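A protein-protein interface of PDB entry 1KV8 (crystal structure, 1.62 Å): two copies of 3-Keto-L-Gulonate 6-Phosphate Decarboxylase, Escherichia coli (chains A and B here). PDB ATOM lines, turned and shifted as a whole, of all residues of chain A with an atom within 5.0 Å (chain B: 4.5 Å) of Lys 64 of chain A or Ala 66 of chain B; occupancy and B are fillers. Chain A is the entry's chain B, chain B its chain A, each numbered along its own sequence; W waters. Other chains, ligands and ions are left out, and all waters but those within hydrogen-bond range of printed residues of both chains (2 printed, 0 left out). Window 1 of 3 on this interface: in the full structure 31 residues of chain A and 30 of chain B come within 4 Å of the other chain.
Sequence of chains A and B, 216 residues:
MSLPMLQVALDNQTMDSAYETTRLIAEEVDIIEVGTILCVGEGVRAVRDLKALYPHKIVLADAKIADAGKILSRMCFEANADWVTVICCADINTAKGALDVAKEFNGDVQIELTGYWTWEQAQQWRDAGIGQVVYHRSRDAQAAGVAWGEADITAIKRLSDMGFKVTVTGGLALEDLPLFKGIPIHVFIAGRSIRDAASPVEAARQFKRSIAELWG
Lys 64 of chain A touches Ala 66 of chain B, and with the chains exchanged Ala 66 of chain A touches Lys 64 of chain B.
Ala 66 of chain A touches Ile 87 of chain B, but with the chains exchanged Ile 87 of chain A does not touch Ala 66 of chain B (4.1 Å).
OG1 of Thr 36 of chain A lies within hydrogen-bond range of NZ of Lys 64 of chain A (2.9 Å).
NZ of Lys 64 of chain A lies within salt-bridge range of OD2 of Asp 62 of chain A (2.9 Å).
N of Lys 64 of chain A sits at hydrogen-bond distance from OG1 of Thr 85 of chain A (2.9 Å).
The side-chain carboxylate (OE2) of Glu 112 of chain A is in salt-bridge range of the side-chain amino group (NZ) of Lys 64 of chain A (3.8 Å).
OE1 of Glu 112 of chain A lies within hydrogen-bond range of OG1 of Thr 114 of chain A (2.6 Å).
The side-chain hydroxyl (OG1) of Thr 114 of chain A lies close to a ring nitrogen (ND1) of His 136 of chain A (3.4 Å).
Lys 64 of chain A touches just one residue of chain B: Ala 66.
Ala 66 of chain B touches two residues of chain A.
Printed residues of chain A within 4 Å of Asp 67 of chain B: Thr 114.
Printed residues of chain A within 4 Å of Ile 87 of chain B: Ala 66 (3.9 Å).
Ile 87 of chain A touches none of the printed residues of chain B.
Thr 36 of chain A touches none of the printed residues of chain B.
The nearest printed residue of chain B that does not touch Lys 64 of chain A is Asp 67 of chain B (5.3 Å).
The nearest residue of chain A that does not touch Ala 66 of chain B is Ile 87 of chain A (4.1 Å).
Lys 64 of chain A touches Ala 66 of chain B (CD to CB, 3.9 Å).
CB of Ala 66 of chain A touches CD of Lys 64 of chain B, 3.9 Å away.
CB of Ala 66 of chain A touches CD1 of Ile 87 of chain B, at 3.9 Å.
Thr 114 of chain A touches Ala 66 of chain B (CG2 to O, 3.4 Å).
Asp 67 of chain B touches Thr 114 of chain A.
Water W2 lies within hydrogen-bond range of the backbone carbonyl oxygen of Lys 64 of chain A and the backbone carbonyl oxygen of Lys 64 of chain B.
Water W1 lies within hydrogen-bond range of OG1 of Thr 114 of chain A, OD2 of Asp 67 of chain B and ND1 of His 136 of chain A.
Hydrophobic or aromatic side chains of chain A within 4 Å of the printed part of chain B: Ala 66.
Of the 7 printed residues of chain B, 4 touch a printed residue of chain A.
Printed residues of chain B that touch a printed residue of chain A: Lys 64, Ala 66, Asp 67 and Ile 87.
Hydrophobic or aromatic side chains of chain B within 4 Å of the printed part of chain A: Ala 66 and Ile 87.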
ATOM      1  N   THR A  36      23.363 -21.365  -9.579  1.00  0.00           N
ATOM      2  CA  THR A  36      22.538 -20.303 -10.130  1.00  0.00           C
ATOM      3  C   THR A  36      23.354 -19.016 -10.257  1.00  0.00           C
ATOM      4  O   THR A  36      23.208 -18.278 -11.228  1.00  0.00           O
ATOM      5  CB  THR A  36      21.308 -20.053  -9.246  1.00  0.00           C
ATOM      6  OG1 THR A  36      20.669 -21.304  -8.964  1.00  0.00           O
ATOM      7  CG2 THR A  36      20.317 -19.150  -9.965  1.00  0.00           C
ATOM      8  N   ASP A  62      21.935 -25.472 -12.597  1.00  0.00           N
ATOM      9  CA  ASP A  62      20.986 -25.057 -11.566  1.00  0.00           C
ATOM     10  C   ASP A  62      20.339 -23.733 -11.963  1.00  0.00           C
ATOM     11  O   ASP A  62      20.545 -22.700 -11.321  1.00  0.00           O
ATOM     12  CB  ASP A  62      21.724 -24.924 -10.225  1.00  0.00           C
ATOM     13  CG  ASP A  62      20.781 -24.885  -9.040  1.00  0.00           C
ATOM     14  OD1 ASP A  62      19.549 -24.936  -9.237  1.00  0.00           O
ATOM     15  OD2 ASP A  62      21.282 -24.808  -7.899  1.00  0.00           O
ATOM     16  N   ALA A  63      19.542 -23.778 -13.027  1.00  0.00           N
ATOM     17  CA  ALA A  63      18.883 -22.589 -13.547  1.00  0.00           C
ATOM     18  C   ALA A  63      17.651 -22.148 -12.769  1.00  0.00           C
ATOM     19  O   ALA A  63      17.213 -21.005 -12.906  1.00  0.00           O
ATOM     20  CB  ALA A  63      18.515 -22.811 -15.014  1.00  0.00           C
ATOM     21  N   LYS A  64      17.099 -23.046 -11.954  1.00  0.00           N
ATOM     22  CA  LYS A  64      15.908 -22.742 -11.167  1.00  0.00           C
ATOM     23  C   LYS A  64      14.834 -22.100 -12.041  1.00  0.00           C
ATOM     24  O   LYS A  64      14.271 -21.053 -11.712  1.00  0.00           O
ATOM     25  CB  LYS A  64      16.263 -21.828  -9.993  1.00  0.00           C
ATOM     26  CG  LYS A  64      17.117 -22.518  -8.936  1.00  0.00           C
ATOM     27  CD  LYS A  64      17.370 -21.606  -7.744  1.00  0.00           C
ATOM     28  CE  LYS A  64      18.009 -22.373  -6.595  1.00  0.00           C
ATOM     29  NZ  LYS A  64      19.346 -22.925  -6.948  1.00  0.00           N
ATOM     30  N   ILE A  65      14.564 -22.763 -13.158  1.00  0.00           N
ATOM     31  CA  ILE A  65      13.576 -22.327 -14.137  1.00  0.00           C
ATOM     32  C   ILE A  65      12.208 -22.098 -13.499  1.00  0.00           C
ATOM     33  O   ILE A  65      11.643 -23.000 -12.874  1.00  0.00           O
ATOM     34  CB  ILE A  65      13.465 -23.378 -15.259  1.00  0.00           C
ATOM     35  CG1 ILE A  65      14.815 -23.491 -15.975  1.00  0.00           C
ATOM     36  CG2 ILE A  65      12.359 -22.994 -16.236  1.00  0.00           C
ATOM     37  CD1 ILE A  65      14.921 -24.658 -16.929  1.00  0.00           C
ATOM     38  N   ALA A  66      11.674 -20.892 -13.673  1.00  0.00           N
ATOM     39  CA  ALA A  66      10.380 -20.529 -13.097  1.00  0.00           C
ATOM     40  C   ALA A  66       9.252 -20.438 -14.120  1.00  0.00           C
ATOM     41  O   ALA A  66       8.077 -20.444 -13.752  1.00  0.00           O
ATOM     42  CB  ALA A  66      10.503 -19.205 -12.358  1.00  0.00           C
ATOM     43  N   THR A  85      17.448 -27.678 -13.258  1.00  0.00           N
ATOM     44  CA  THR A  85      16.529 -27.518 -12.139  1.00  0.00           C
ATOM     45  C   THR A  85      15.408 -26.548 -12.466  1.00  0.00           C
ATOM     46  O   THR A  85      15.602 -25.567 -13.185  1.00  0.00           O
ATOM     47  CB  THR A  85      17.230 -27.002 -10.854  1.00  0.00           C
ATOM     48  OG1 THR A  85      17.809 -25.715 -11.098  1.00  0.00           O
ATOM     49  CG2 THR A  85      18.312 -27.978 -10.404  1.00  0.00           C
ATOM     50  N   VAL A  86      14.232 -26.851 -11.926  1.00  0.00           N
ATOM     51  CA  VAL A  86      13.032 -26.033 -12.082  1.00  0.00           C
ATOM     52  C   VAL A  86      12.632 -25.652 -10.654  1.00  0.00           C
ATOM     53  O   VAL A  86      12.540 -26.519  -9.786  1.00  0.00           O
ATOM     54  CB  VAL A  86      11.894 -26.852 -12.743  1.00  0.00           C
ATOM     55  CG1 VAL A  86      10.565 -26.099 -12.637  1.00  0.00           C
ATOM     56  CG2 VAL A  86      12.239 -27.128 -14.208  1.00  0.00           C
ATOM     57  N   ILE A  87      12.411 -24.364 -10.403  1.00  0.00           N
ATOM     58  CA  ILE A  87      12.048 -23.923  -9.060  1.00  0.00           C
ATOM     59  C   ILE A  87      10.663 -24.458  -8.670  1.00  0.00           C
ATOM     60  O   ILE A  87       9.759 -24.542  -9.500  1.00  0.00           O
ATOM     61  CB  ILE A  87      12.107 -22.377  -8.946  1.00  0.00           C
ATOM     62  CG1 ILE A  87      12.126 -21.964  -7.472  1.00  0.00           C
ATOM     63  CG2 ILE A  87      10.931 -21.743  -9.669  1.00  0.00           C
ATOM     64  CD1 ILE A  87      13.351 -22.455  -6.708  1.00  0.00           C
ATOM     65  N   GLU A 112      13.703 -27.859  -7.657  1.00  0.00           N
ATOM     66  CA  GLU A 112      14.505 -27.240  -6.607  1.00  0.00           C
ATOM     67  C   GLU A 112      13.580 -26.735  -5.508  1.00  0.00           C
ATOM     68  O   GLU A 112      12.804 -25.799  -5.716  1.00  0.00           O
ATOM     69  CB  GLU A 112      15.323 -26.078  -7.189  1.00  0.00           C
ATOM     70  CG  GLU A 112      16.834 -26.165  -6.934  1.00  0.00           C
ATOM     71  CD  GLU A 112      17.203 -25.974  -5.474  1.00  0.00           C
ATOM     72  OE1 GLU A 112      16.313 -25.617  -4.679  1.00  0.00           O
ATOM     73  OE2 GLU A 112      18.389 -26.171  -5.127  1.00  0.00           O
ATOM     74  N   THR A 114      13.625 -24.728  -2.963  1.00  0.00           N
ATOM     75  CA  THR A 114      14.163 -23.583  -2.247  1.00  0.00           C
ATOM     76  C   THR A 114      12.974 -22.648  -2.099  1.00  0.00           C
ATOM     77  O   THR A 114      12.401 -22.199  -3.093  1.00  0.00           O
ATOM     78  CB  THR A 114      15.274 -22.859  -3.038  1.00  0.00           C
ATOM     79  OG1 THR A 114      16.464 -23.658  -3.038  1.00  0.00           O
ATOM     80  CG2 THR A 114      15.582 -21.503  -2.405  1.00  0.00           C
ATOM     81  N   HIS A 136      16.304 -28.163  -0.226  1.00  0.00           N
ATOM     82  CA  HIS A 136      17.281 -27.117   0.002  1.00  0.00           C
ATOM     83  C   HIS A 136      16.979 -26.121   1.110  1.00  0.00           C
ATOM     84  O   HIS A 136      16.020 -25.358   1.028  1.00  0.00           O
ATOM     85  CB  HIS A 136      17.461 -26.371  -1.325  1.00  0.00           C
ATOM     86  CG  HIS A 136      18.756 -25.635  -1.449  1.00  0.00           C
ATOM     87  ND1 HIS A 136      19.361 -25.412  -2.669  1.00  0.00           N
ATOM     88  CD2 HIS A 136      19.558 -25.064  -0.521  1.00  0.00           C
ATOM     89  CE1 HIS A 136      20.482 -24.739  -2.484  1.00  0.00           C
ATOM     90  NE2 HIS A 136      20.625 -24.514  -1.189  1.00  0.00           N
ATOM     91  N   LYS B  64      14.846 -13.185 -11.266  1.00  0.00           N
ATOM     92  CA  LYS B  64      13.976 -14.076 -10.505  1.00  0.00           C
ATOM     93  C   LYS B  64      14.779 -14.793  -9.419  1.00  0.00           C
ATOM     94  O   LYS B  64      14.759 -16.023  -9.299  1.00  0.00           O
ATOM     95  CB  LYS B  64      13.297 -15.081 -11.442  1.00  0.00           C
ATOM     96  CG  LYS B  64      12.228 -14.446 -12.337  1.00  0.00           C
ATOM     97  CD  LYS B  64      11.485 -15.477 -13.178  1.00  0.00           C
ATOM     98  CE  LYS B  64      10.331 -14.830 -13.940  1.00  0.00           C
ATOM     99  NZ  LYS B  64      10.810 -13.791 -14.895  1.00  0.00           N
ATOM    100  N   ILE B  65      15.484 -13.992  -8.631  1.00  0.00           N
ATOM    101  CA  ILE B  65      16.319 -14.479  -7.536  1.00  0.00           C
ATOM    102  C   ILE B  65      15.515 -15.364  -6.585  1.00  0.00           C
ATOM    103  O   ILE B  65      14.458 -14.969  -6.097  1.00  0.00           O
ATOM    104  CB  ILE B  65      16.919 -13.285  -6.763  1.00  0.00           C
ATOM    105  CG1 ILE B  65      17.823 -12.473  -7.697  1.00  0.00           C
ATOM    106  CG2 ILE B  65      17.700 -13.779  -5.550  1.00  0.00           C
ATOM    107  CD1 ILE B  65      18.219 -11.124  -7.150  1.00  0.00           C
ATOM    108  N   ALA B  66      16.025 -16.567  -6.325  1.00  0.00           N
ATOM    109  CA  ALA B  66      15.335 -17.511  -5.450  1.00  0.00           C
ATOM    110  C   ALA B  66      16.025 -17.712  -4.108  1.00  0.00           C
ATOM    111  O   ALA B  66      15.418 -18.212  -3.164  1.00  0.00           O
ATOM    112  CB  ALA B  66      15.185 -18.854  -6.156  1.00  0.00           C
ATOM    113  N   ASP B  67      17.292 -17.324  -4.031  1.00  0.00           N
ATOM    114  CA  ASP B  67      18.074 -17.476  -2.810  1.00  0.00           C
ATOM    115  C   ASP B  67      19.355 -16.665  -3.002  1.00  0.00           C
ATOM    116  O   ASP B  67      19.622 -16.185  -4.104  1.00  0.00           O
ATOM    117  CB  ASP B  67      18.389 -18.963  -2.586  1.00  0.00           C
ATOM    118  CG  ASP B  67      18.945 -19.250  -1.198  1.00  0.00           C
ATOM    119  OD1 ASP B  67      18.817 -18.384  -0.309  1.00  0.00           O
ATOM    120  OD2 ASP B  67      19.503 -20.353  -0.996  1.00  0.00           O
ATOM    121  N   ILE B  87      11.910 -14.126  -7.169  1.00  0.00           N
ATOM    122  CA  ILE B  87      10.776 -15.014  -7.400  1.00  0.00           C
ATOM    123  C   ILE B  87       9.897 -15.108  -6.144  1.00  0.00           C
ATOM    124  O   ILE B  87      10.393 -15.097  -5.017  1.00  0.00           O
ATOM    125  CB  ILE B  87      11.252 -16.412  -7.859  1.00  0.00           C
ATOM    126  CG1 ILE B  87      10.069 -17.208  -8.420  1.00  0.00           C
ATOM    127  CG2 ILE B  87      11.922 -17.144  -6.711  1.00  0.00           C
ATOM    128  CD1 ILE B  87       9.446 -16.593  -9.672  1.00  0.00           C
ATOM    129  N   ALA B  90      10.562 -17.436  -2.915  1.00  0.00           N
ATOM    130  CA  ALA B  90      11.786 -17.263  -2.137  1.00  0.00           C
ATOM    131  C   ALA B  90      11.524 -17.028  -0.656  1.00  0.00           C
ATOM    132  O   ALA B  90      10.507 -16.449  -0.269  1.00  0.00           O
ATOM    133  CB  ALA B  90      12.608 -16.107  -2.702  1.00  0.00           C
ATOM    134  N   THR B  94      15.338 -13.721   1.598  1.00  0.00           N
ATOM    135  CA  THR B  94      15.954 -13.493   0.296  1.00  0.00           C
ATOM    136  C   THR B  94      15.490 -12.134  -0.231  1.00  0.00           C
ATOM    137  O   THR B  94      16.297 -11.337  -0.708  1.00  0.00           O
ATOM    138  CB  THR B  94      15.578 -14.611  -0.691  1.00  0.00           C
ATOM    139  OG1 THR B  94      16.106 -15.852  -0.211  1.00  0.00           O
ATOM    140  CG2 THR B  94      16.143 -14.325  -2.080  1.00  0.00           C
HETATM  141  O   HOH W   1      18.847 -22.253  -3.111  1.00  0.00           O
HETATM  142  O   HOH W   2      13.627 -18.455 -11.068  1.00  0.00           O
